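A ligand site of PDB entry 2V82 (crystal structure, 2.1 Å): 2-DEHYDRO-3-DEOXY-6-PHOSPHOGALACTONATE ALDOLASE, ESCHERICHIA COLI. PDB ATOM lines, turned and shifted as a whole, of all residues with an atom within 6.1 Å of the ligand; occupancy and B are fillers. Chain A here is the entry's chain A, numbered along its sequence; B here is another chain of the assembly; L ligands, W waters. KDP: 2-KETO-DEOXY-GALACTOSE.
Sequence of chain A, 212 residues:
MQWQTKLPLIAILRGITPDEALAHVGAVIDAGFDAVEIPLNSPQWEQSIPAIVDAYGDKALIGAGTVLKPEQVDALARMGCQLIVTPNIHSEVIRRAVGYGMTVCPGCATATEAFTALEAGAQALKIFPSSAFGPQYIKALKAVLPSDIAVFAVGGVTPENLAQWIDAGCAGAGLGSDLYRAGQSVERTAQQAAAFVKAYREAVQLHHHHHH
NZ of Lys 126 is bonded to CAM of the ligand, at 1.3 Å.
An oxygen (OAA) of the ligand lies close to the backbone NH of Thr 86 (3.3 Å).
The side-chain hydroxyl (OG) of Ser 177 sits at hydrogen-bond distance from an oxygen (OAG) of the ligand.
N of Ser 177 sits at hydrogen-bond distance from OAG of the ligand (2.9 Å).
N of Thr 66 is in hydrogen-bond range of OAA of the ligand (3.0 Å).
The guanidinium group (NH2) of Arg 14 is in salt-bridge range of an oxygen (OAF) of the ligand (2.7 Å).
OG1 of Thr 66 lies within hydrogen-bond range of OAF of the ligand (2.9 Å).
The backbone NH of Gly 176 sits at hydrogen-bond distance from an oxygen (OAC) of the ligand.
The backbone NH of Gly 65 sits at hydrogen-bond distance from the side-chain carboxylate of Glu 37, 3.0 Å away.
The backbone carbonyl oxygen (O) of Leu 175 is in hydrogen-bond range of the backbone NH (N) of Ile 12, 2.9 Å away.
O of Asn 88 is in hydrogen-bond range of OG1 of Thr 86, 2.5 Å away.
The backbone NH of Val 85 sits at hydrogen-bond distance from the backbone carbonyl oxygen of Ala 64 (2.8 Å).
NH1 of Arg 14 sits at hydrogen-bond distance from O of Ala 143 of chain B (3.1 Å).
N of Thr 66 sits at hydrogen-bond distance from O of Val 85.
The side-chain amino group of Lys 126 sits at hydrogen-bond distance from the backbone carbonyl oxygen of Thr 86 (3.0 Å).
The guanidinium group (NH1) of Arg 14 is in hydrogen-bond range of the side-chain hydroxyl (OG1) of Thr 66.
The backbone carbonyl oxygen (O) of Val 85 lies close to an oxygen (OAA) of the ligand, 3.5 Å away.
The backbone nitrogen (N) of Pro 87 lies close to an oxygen (OAA) of the ligand (3.4 Å).
Merely in contact with the ligand: Ile 12 (3.5 Å), Gly 65 (3.9 Å), Phe 128 (3.3 Å), Val 154 (3.6 Å), Gly 155 (3.6 Å) and Gly 156 (3.6 Å).
Hydrophobic or aromatic side chains that line the ligand: Ile 12, Val 85, Pro 87, Phe 128 and Val 154.
14 residues have an atom within 4 Å of the ligand: Ile 12, Arg 14, Gly 65, Thr 66, Val 85, Thr 86, Pro 87, Lys 126, Phe 128, Val 154, Gly 155, Gly 156, Gly 176 and Ser 177.
The nearest printed residue that does not touch the ligand is Val 144 of chain B (4.1 Å).
Water W1 lies within hydrogen-bond range of an oxygen (OAC) of the ligand (2.7 Å), the backbone carbonyl oxygen (O) of Val 157 (3.2 Å), the side-chain carboxylate (OD2) of Asp 178 (3.3 Å) and the backbone NH (N) of Gly 176 (3.3 Å).
Water W2 lies within hydrogen-bond range of the backbone carbonyl oxygen of Gly 174 (2.6 Å), an oxygen (OAC) of the ligand (2.7 Å) and the backbone NH of Gly 155 (2.8 Å).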
ATOM      1  N   ILE A  12     -32.049  -6.653  23.656  1.00  0.00           N
ATOM      2  CA  ILE A  12     -32.119  -6.246  22.258  1.00  0.00           C
ATOM      3  C   ILE A  12     -32.759  -7.369  21.465  1.00  0.00           C
ATOM      4  O   ILE A  12     -32.203  -8.454  21.370  1.00  0.00           O
ATOM      5  CB  ILE A  12     -30.727  -5.903  21.718  1.00  0.00           C
ATOM      6  CG1 ILE A  12     -30.118  -4.746  22.539  1.00  0.00           C
ATOM      7  CG2 ILE A  12     -30.768  -5.544  20.201  1.00  0.00           C
ATOM      8  CD1 ILE A  12     -28.594  -4.688  22.392  1.00  0.00           C
ATOM      9  N   ARG A  14     -33.619  -8.282  18.110  1.00  0.00           N
ATOM     10  CA  ARG A  14     -33.466  -8.044  16.682  1.00  0.00           C
ATOM     11  C   ARG A  14     -34.267  -9.093  15.906  1.00  0.00           C
ATOM     12  O   ARG A  14     -34.103 -10.293  16.163  1.00  0.00           O
ATOM     13  CB  ARG A  14     -31.975  -8.070  16.265  1.00  0.00           C
ATOM     14  CG  ARG A  14     -31.765  -7.763  14.761  1.00  0.00           C
ATOM     15  CD  ARG A  14     -30.329  -7.549  14.401  1.00  0.00           C
ATOM     16  NE  ARG A  14     -29.671  -6.667  15.370  1.00  0.00           N
ATOM     17  CZ  ARG A  14     -29.506  -5.353  15.218  1.00  0.00           C
ATOM     18  NH1 ARG A  14     -29.912  -4.737  14.107  1.00  0.00           N
ATOM     19  NH2 ARG A  14     -28.919  -4.673  16.174  1.00  0.00           N
ATOM     20  N   GLU A  37     -35.253  -2.816  23.740  1.00  0.00           N
ATOM     21  CA  GLU A  37     -35.299  -2.104  22.486  1.00  0.00           C
ATOM     22  C   GLU A  37     -35.471  -3.087  21.336  1.00  0.00           C
ATOM     23  O   GLU A  37     -35.030  -4.241  21.400  1.00  0.00           O
ATOM     24  CB  GLU A  37     -34.050  -1.228  22.305  1.00  0.00           C
ATOM     25  CG  GLU A  37     -32.715  -1.996  22.190  1.00  0.00           C
ATOM     26  CD  GLU A  37     -32.211  -2.145  20.756  1.00  0.00           C
ATOM     27  OE1 GLU A  37     -30.974  -2.036  20.541  1.00  0.00           O
ATOM     28  OE2 GLU A  37     -33.033  -2.370  19.819  1.00  0.00           O
ATOM     29  N   PRO A  39     -34.588  -3.294  17.380  1.00  0.00           N
ATOM     30  CA  PRO A  39     -33.894  -2.729  16.202  1.00  0.00           C
ATOM     31  C   PRO A  39     -34.828  -2.446  15.015  1.00  0.00           C
ATOM     32  O   PRO A  39     -35.776  -3.201  14.772  1.00  0.00           O
ATOM     33  CB  PRO A  39     -32.879  -3.820  15.847  1.00  0.00           C
ATOM     34  CG  PRO A  39     -32.588  -4.486  17.195  1.00  0.00           C
ATOM     35  CD  PRO A  39     -33.958  -4.561  17.817  1.00  0.00           C
ATOM     36  N   ALA A  64     -35.841   1.747  20.763  1.00  0.00           N
ATOM     37  CA  ALA A  64     -35.488   1.222  19.461  1.00  0.00           C
ATOM     38  C   ALA A  64     -33.986   1.175  19.267  1.00  0.00           C
ATOM     39  O   ALA A  64     -33.247   1.963  19.870  1.00  0.00           O
ATOM     40  CB  ALA A  64     -36.135   2.059  18.382  1.00  0.00           C
ATOM     41  N   GLY A  65     -33.541   0.267  18.404  1.00  0.00           N
ATOM     42  CA  GLY A  65     -32.134   0.158  18.056  1.00  0.00           C
ATOM     43  C   GLY A  65     -31.937   0.382  16.582  1.00  0.00           C
ATOM     44  O   GLY A  65     -32.899   0.551  15.821  1.00  0.00           O
ATOM     45  N   THR A  66     -30.665   0.379  16.165  1.00  0.00           N
ATOM     46  CA  THR A  66     -30.283   0.537  14.759  1.00  0.00           C
ATOM     47  C   THR A  66     -30.985   1.756  14.121  1.00  0.00           C
ATOM     48  O   THR A  66     -31.499   1.710  12.985  1.00  0.00           O
ATOM     49  CB  THR A  66     -30.535  -0.773  13.942  1.00  0.00           C
ATOM     50  OG1 THR A  66     -30.372  -1.914  14.807  1.00  0.00           O
ATOM     51  CG2 THR A  66     -29.525  -0.904  12.755  1.00  0.00           C
ATOM     52  N   VAL A  67     -30.951   2.854  14.888  1.00  0.00           N
ATOM     53  CA  VAL A  67     -31.571   4.100  14.501  1.00  0.00           C
ATOM     54  C   VAL A  67     -30.540   4.945  13.752  1.00  0.00           C
ATOM     55  O   VAL A  67     -29.622   5.486  14.373  1.00  0.00           O
ATOM     56  CB  VAL A  67     -32.094   4.877  15.763  1.00  0.00           C
ATOM     57  CG1 VAL A  67     -32.739   6.190  15.339  1.00  0.00           C
ATOM     58  CG2 VAL A  67     -33.061   4.009  16.567  1.00  0.00           C
ATOM     59  N   VAL A  85     -31.070   3.535  20.776  1.00  0.00           N
ATOM     60  CA  VAL A  85     -29.790   2.842  20.672  1.00  0.00           C
ATOM     61  C   VAL A  85     -29.391   2.777  19.201  1.00  0.00           C
ATOM     62  O   VAL A  85     -30.259   2.606  18.327  1.00  0.00           O
ATOM     63  CB  VAL A  85     -29.901   1.385  21.245  1.00  0.00           C
ATOM     64  CG1 VAL A  85     -28.539   0.698  21.283  1.00  0.00           C
ATOM     65  CG2 VAL A  85     -30.512   1.406  22.624  1.00  0.00           C
ATOM     66  N   THR A  86     -28.078   2.903  18.931  1.00  0.00           N
ATOM     67  CA  THR A  86     -27.539   2.976  17.566  1.00  0.00           C
ATOM     68  C   THR A  86     -26.299   2.082  17.449  1.00  0.00           C
ATOM     69  O   THR A  86     -25.675   1.742  18.458  1.00  0.00           O
ATOM     70  CB  THR A  86     -27.172   4.417  17.121  1.00  0.00           C
ATOM     71  OG1 THR A  86     -25.969   4.839  17.781  1.00  0.00           O
ATOM     72  CG2 THR A  86     -28.284   5.410  17.432  1.00  0.00           C
ATOM     73  N   PRO A  87     -25.953   1.655  16.228  1.00  0.00           N
ATOM     74  CA  PRO A  87     -24.670   0.970  16.057  1.00  0.00           C
ATOM     75  C   PRO A  87     -23.520   1.940  15.803  1.00  0.00           C
ATOM     76  O   PRO A  87     -22.346   1.574  15.902  1.00  0.00           O
ATOM     77  CB  PRO A  87     -24.891   0.089  14.835  1.00  0.00           C
ATOM     78  CG  PRO A  87     -26.069   0.687  14.092  1.00  0.00           C
ATOM     79  CD  PRO A  87     -26.717   1.731  14.968  1.00  0.00           C
ATOM     80  N   ASN A  88     -23.854   3.199  15.504  1.00  0.00           N
ATOM     81  CA  ASN A  88     -22.870   4.183  15.063  1.00  0.00           C
ATOM     82  C   ASN A  88     -23.094   5.557  15.700  1.00  0.00           C
ATOM     83  O   ASN A  88     -24.153   5.812  16.302  1.00  0.00           O
ATOM     84  CB  ASN A  88     -22.938   4.306  13.547  1.00  0.00           C
ATOM     85  CG  ASN A  88     -24.277   4.841  13.076  1.00  0.00           C
ATOM     86  OD1 ASN A  88     -25.309   4.612  13.722  1.00  0.00           O
ATOM     87  ND2 ASN A  88     -24.276   5.563  11.949  1.00  0.00           N
ATOM     88  N   CYS A 105     -28.281   5.922  23.840  1.00  0.00           N
ATOM     89  CA  CYS A 105     -27.096   5.137  24.076  1.00  0.00           C
ATOM     90  C   CYS A 105     -26.497   4.782  22.725  1.00  0.00           C
ATOM     91  O   CYS A 105     -26.702   3.676  22.208  1.00  0.00           O
ATOM     92  CB  CYS A 105     -27.400   3.868  24.898  1.00  0.00           C
ATOM     93  SG  CYS A 105     -25.897   2.988  25.466  1.00  0.00           S
ATOM     94  N   LYS A 126     -22.355   3.159  24.003  1.00  0.00           N
ATOM     95  CA  LYS A 126     -22.367   1.735  23.682  1.00  0.00           C
ATOM     96  C   LYS A 126     -21.044   1.488  22.974  1.00  0.00           C
ATOM     97  O   LYS A 126     -20.709   2.195  22.022  1.00  0.00           O
ATOM     98  CB  LYS A 126     -23.589   1.418  22.788  1.00  0.00           C
ATOM     99  CG  LYS A 126     -23.621   0.063  22.032  1.00  0.00           C
ATOM    100  CD  LYS A 126     -24.560   0.102  20.807  1.00  0.00           C
ATOM    101  CE  LYS A 126     -24.688  -1.207  19.965  1.00  0.00           C
ATOM    102  NZ  LYS A 126     -25.980  -1.142  19.127  1.00  0.00           N
ATOM    103  N   PHE A 128     -19.468  -0.884  20.512  1.00  0.00           N
ATOM    104  CA  PHE A 128     -19.969  -1.907  19.615  1.00  0.00           C
ATOM    105  C   PHE A 128     -19.079  -2.129  18.392  1.00  0.00           C
ATOM    106  O   PHE A 128     -18.673  -1.163  17.743  1.00  0.00           O
ATOM    107  CB  PHE A 128     -21.404  -1.580  19.195  1.00  0.00           C
ATOM    108  CG  PHE A 128     -21.865  -2.366  18.030  1.00  0.00           C
ATOM    109  CD1 PHE A 128     -22.255  -3.699  18.197  1.00  0.00           C
ATOM    110  CD2 PHE A 128     -21.884  -1.804  16.748  1.00  0.00           C
ATOM    111  CE1 PHE A 128     -22.659  -4.450  17.097  1.00  0.00           C
ATOM    112  CE2 PHE A 128     -22.278  -2.552  15.647  1.00  0.00           C
ATOM    113  CZ  PHE A 128     -22.675  -3.864  15.817  1.00  0.00           C
ATOM    114  N   PRO A 129     -18.762  -3.396  18.084  1.00  0.00           N
ATOM    115  CA  PRO A 129     -18.938  -4.605  18.912  1.00  0.00           C
ATOM    116  C   PRO A 129     -17.795  -4.791  19.926  1.00  0.00           C
ATOM    117  O   PRO A 129     -16.620  -4.778  19.551  1.00  0.00           O
ATOM    118  CB  PRO A 129     -18.951  -5.753  17.888  1.00  0.00           C
ATOM    119  CG  PRO A 129     -18.905  -5.089  16.518  1.00  0.00           C
ATOM    120  CD  PRO A 129     -18.291  -3.746  16.745  1.00  0.00           C
ATOM    121  N   VAL A 154     -21.641  -3.990  24.204  1.00  0.00           N
ATOM    122  CA  VAL A 154     -22.612  -4.646  23.313  1.00  0.00           C
ATOM    123  C   VAL A 154     -21.827  -5.381  22.234  1.00  0.00           C
ATOM    124  O   VAL A 154     -21.020  -4.774  21.518  1.00  0.00           O
ATOM    125  CB  VAL A 154     -23.575  -3.667  22.622  1.00  0.00           C
ATOM    126  CG1 VAL A 154     -24.462  -4.440  21.620  1.00  0.00           C
ATOM    127  CG2 VAL A 154     -24.442  -2.929  23.610  1.00  0.00           C
ATOM    128  N   GLY A 155     -22.052  -6.689  22.144  1.00  0.00           N
ATOM    129  CA  GLY A 155     -21.447  -7.510  21.097  1.00  0.00           C
ATOM    130  C   GLY A 155     -20.658  -8.614  21.718  1.00  0.00           C
ATOM    131  O   GLY A 155     -19.603  -8.372  22.288  1.00  0.00           O
ATOM    132  N   GLY A 156     -21.177  -9.836  21.623  1.00  0.00           N
ATOM    133  CA  GLY A 156     -20.532 -11.015  22.242  1.00  0.00           C
ATOM    134  C   GLY A 156     -20.432 -11.010  23.765  1.00  0.00           C
ATOM    135  O   GLY A 156     -19.481 -11.564  24.338  1.00  0.00           O
ATOM    136  N   VAL A 157     -21.409 -10.385  24.425  1.00  0.00           N
ATOM    137  CA  VAL A 157     -21.551 -10.457  25.888  1.00  0.00           C
ATOM    138  C   VAL A 157     -22.452 -11.643  26.260  1.00  0.00           C
ATOM    139  O   VAL A 157     -23.555 -11.804  25.710  1.00  0.00           O
ATOM    140  CB  VAL A 157     -22.137  -9.149  26.486  1.00  0.00           C
ATOM    141  CG1 VAL A 157     -22.160  -9.215  28.029  1.00  0.00           C
ATOM    142  CG2 VAL A 157     -21.340  -7.929  26.010  1.00  0.00           C
ATOM    143  N   GLY A 174     -25.684  -4.333  26.632  1.00  0.00           N
ATOM    144  CA  GLY A 174     -26.782  -4.582  25.710  1.00  0.00           C
ATOM    145  C   GLY A 174     -26.620  -5.999  25.192  1.00  0.00           C
ATOM    146  O   GLY A 174     -25.543  -6.377  24.723  1.00  0.00           O
ATOM    147  N   LEU A 175     -27.680  -6.791  25.299  1.00  0.00           N
ATOM    148  CA  LEU A 175     -27.633  -8.207  24.946  1.00  0.00           C
ATOM    149  C   LEU A 175     -28.529  -8.546  23.759  1.00  0.00           C
ATOM    150  O   LEU A 175     -29.747  -8.336  23.791  1.00  0.00           O
ATOM    151  CB  LEU A 175     -27.988  -9.055  26.163  1.00  0.00           C
ATOM    152  CG  LEU A 175     -27.325  -8.478  27.419  1.00  0.00           C
ATOM    153  CD1 LEU A 175     -28.092  -8.882  28.638  1.00  0.00           C
ATOM    154  CD2 LEU A 175     -25.844  -8.857  27.466  1.00  0.00           C
ATOM    155  N   GLY A 176     -27.901  -9.057  22.703  1.00  0.00           N
ATOM    156  CA  GLY A 176     -28.596  -9.284  21.443  1.00  0.00           C
ATOM    157  C   GLY A 176     -28.826 -10.765  21.205  1.00  0.00           C
ATOM    158  O   GLY A 176     -29.628 -11.392  21.896  1.00  0.00           O
ATOM    159  N   SER A 177     -28.098 -11.309  20.232  1.00  0.00           N
ATOM    160  CA  SER A 177     -28.231 -12.708  19.797  1.00  0.00           C
ATOM    161  C   SER A 177     -28.119 -13.739  20.929  1.00  0.00           C
ATOM    162  O   SER A 177     -28.698 -14.808  20.847  1.00  0.00           O
ATOM    163  CB  SER A 177     -27.204 -13.025  18.725  1.00  0.00           C
ATOM    164  OG  SER A 177     -25.926 -12.539  19.108  1.00  0.00           O
ATOM    165  N   ASP A 178     -27.378 -13.404  21.991  1.00  0.00           N
ATOM    166  CA  ASP A 178     -27.149 -14.343  23.105  1.00  0.00           C
ATOM    167  C   ASP A 178     -28.358 -14.366  24.028  1.00  0.00           C
ATOM    168  O   ASP A 178     -28.509 -15.270  24.861  1.00  0.00           O
ATOM    169  CB  ASP A 178     -25.895 -13.959  23.880  1.00  0.00           C
ATOM    170  CG  ASP A 178     -24.622 -14.624  23.337  1.00  0.00           C
ATOM    171  OD1 ASP A 178     -24.539 -15.880  23.385  1.00  0.00           O
ATOM    172  OD2 ASP A 178     -23.695 -13.884  22.878  1.00  0.00           O
ATOM    173  N   GLN B 136     -15.662 -12.623  13.598  1.00  0.00           N
ATOM    174  CA  GLN B 136     -16.792 -12.292  14.456  1.00  0.00           C
ATOM    175  C   GLN B 136     -17.142 -10.813  14.383  1.00  0.00           C
ATOM    176  O   GLN B 136     -18.303 -10.432  14.537  1.00  0.00           O
ATOM    177  CB  GLN B 136     -16.525 -12.708  15.912  1.00  0.00           C
ATOM    178  CG  GLN B 136     -17.657 -12.410  16.889  1.00  0.00           C
ATOM    179  CD  GLN B 136     -18.909 -13.244  16.605  1.00  0.00           C
ATOM    180  OE1 GLN B 136     -18.834 -14.466  16.373  1.00  0.00           O
ATOM    181  NE2 GLN B 136     -20.080 -12.574  16.638  1.00  0.00           N
ATOM    182  N   ALA B 140     -20.757  -9.405  13.430  1.00  0.00           N
ATOM    183  CA  ALA B 140     -21.442  -8.393  14.230  1.00  0.00           C
ATOM    184  C   ALA B 140     -21.832  -7.171  13.374  1.00  0.00           C
ATOM    185  O   ALA B 140     -22.915  -6.618  13.520  1.00  0.00           O
ATOM    186  CB  ALA B 140     -20.596  -7.997  15.436  1.00  0.00           C
ATOM    187  N   ALA B 143     -24.938  -7.668  11.187  1.00  0.00           N
ATOM    188  CA  ALA B 143     -26.250  -7.631  11.813  1.00  0.00           C
ATOM    189  C   ALA B 143     -26.872  -6.219  11.760  1.00  0.00           C
ATOM    190  O   ALA B 143     -28.079  -6.072  11.966  1.00  0.00           O
ATOM    191  CB  ALA B 143     -26.188  -8.170  13.228  1.00  0.00           C
ATOM    192  N   VAL B 144     -26.048  -5.200  11.468  1.00  0.00           N
ATOM    193  CA  VAL B 144     -26.576  -3.838  11.290  1.00  0.00           C
ATOM    194  C   VAL B 144     -26.530  -3.284   9.844  1.00  0.00           C
ATOM    195  O   VAL B 144     -27.318  -2.417   9.483  1.00  0.00           O
ATOM    196  CB  VAL B 144     -25.964  -2.810  12.299  1.00  0.00           C
ATOM    197  CG1 VAL B 144     -26.269  -3.225  13.731  1.00  0.00           C
ATOM    198  CG2 VAL B 144     -24.475  -2.629  12.093  1.00  0.00           C
HETATM  199  OAH KDP L   1     -23.792  -9.426  19.134  1.00  0.00           O
HETATM  200  PAP KDP L   1     -25.092  -8.840  19.673  1.00  0.00           P
HETATM  201  OAC KDP L   1     -25.216  -9.186  21.143  1.00  0.00           O
HETATM  202  OAG KDP L   1     -26.265  -9.458  18.948  1.00  0.00           O
HETATM  203  OAK KDP L   1     -25.121  -7.235  19.486  1.00  0.00           O
HETATM  204  CAI KDP L   1     -24.824  -6.636  18.208  1.00  0.00           C
HETATM  205  CAN KDP L   1     -26.023  -5.879  17.630  1.00  0.00           C
HETATM  206  OAD KDP L   1     -27.106  -6.799  17.548  1.00  0.00           O
HETATM  207  CAO KDP L   1     -26.364  -4.623  18.475  1.00  0.00           C
HETATM  208  OAE KDP L   1     -27.740  -4.594  18.737  1.00  0.00           O
HETATM  209  CAJ KDP L   1     -25.973  -3.303  17.789  1.00  0.00           C
HETATM  210  CAM KDP L   1     -26.562  -1.944  18.260  1.00  0.00           C
HETATM  211  CAL KDP L   1     -27.913  -1.427  17.699  1.00  0.00           C
HETATM  212  OAA KDP L   1     -28.280  -0.233  17.839  1.00  0.00           O
HETATM  213  OAF KDP L   1     -28.677  -2.170  17.088  1.00  0.00           O
HETATM  214  O   HOH W   1     -25.178 -10.930  23.148  1.00  0.00           O
HETATM  215  O   HOH W   2     -24.104  -8.170  23.415  1.00  0.00           O
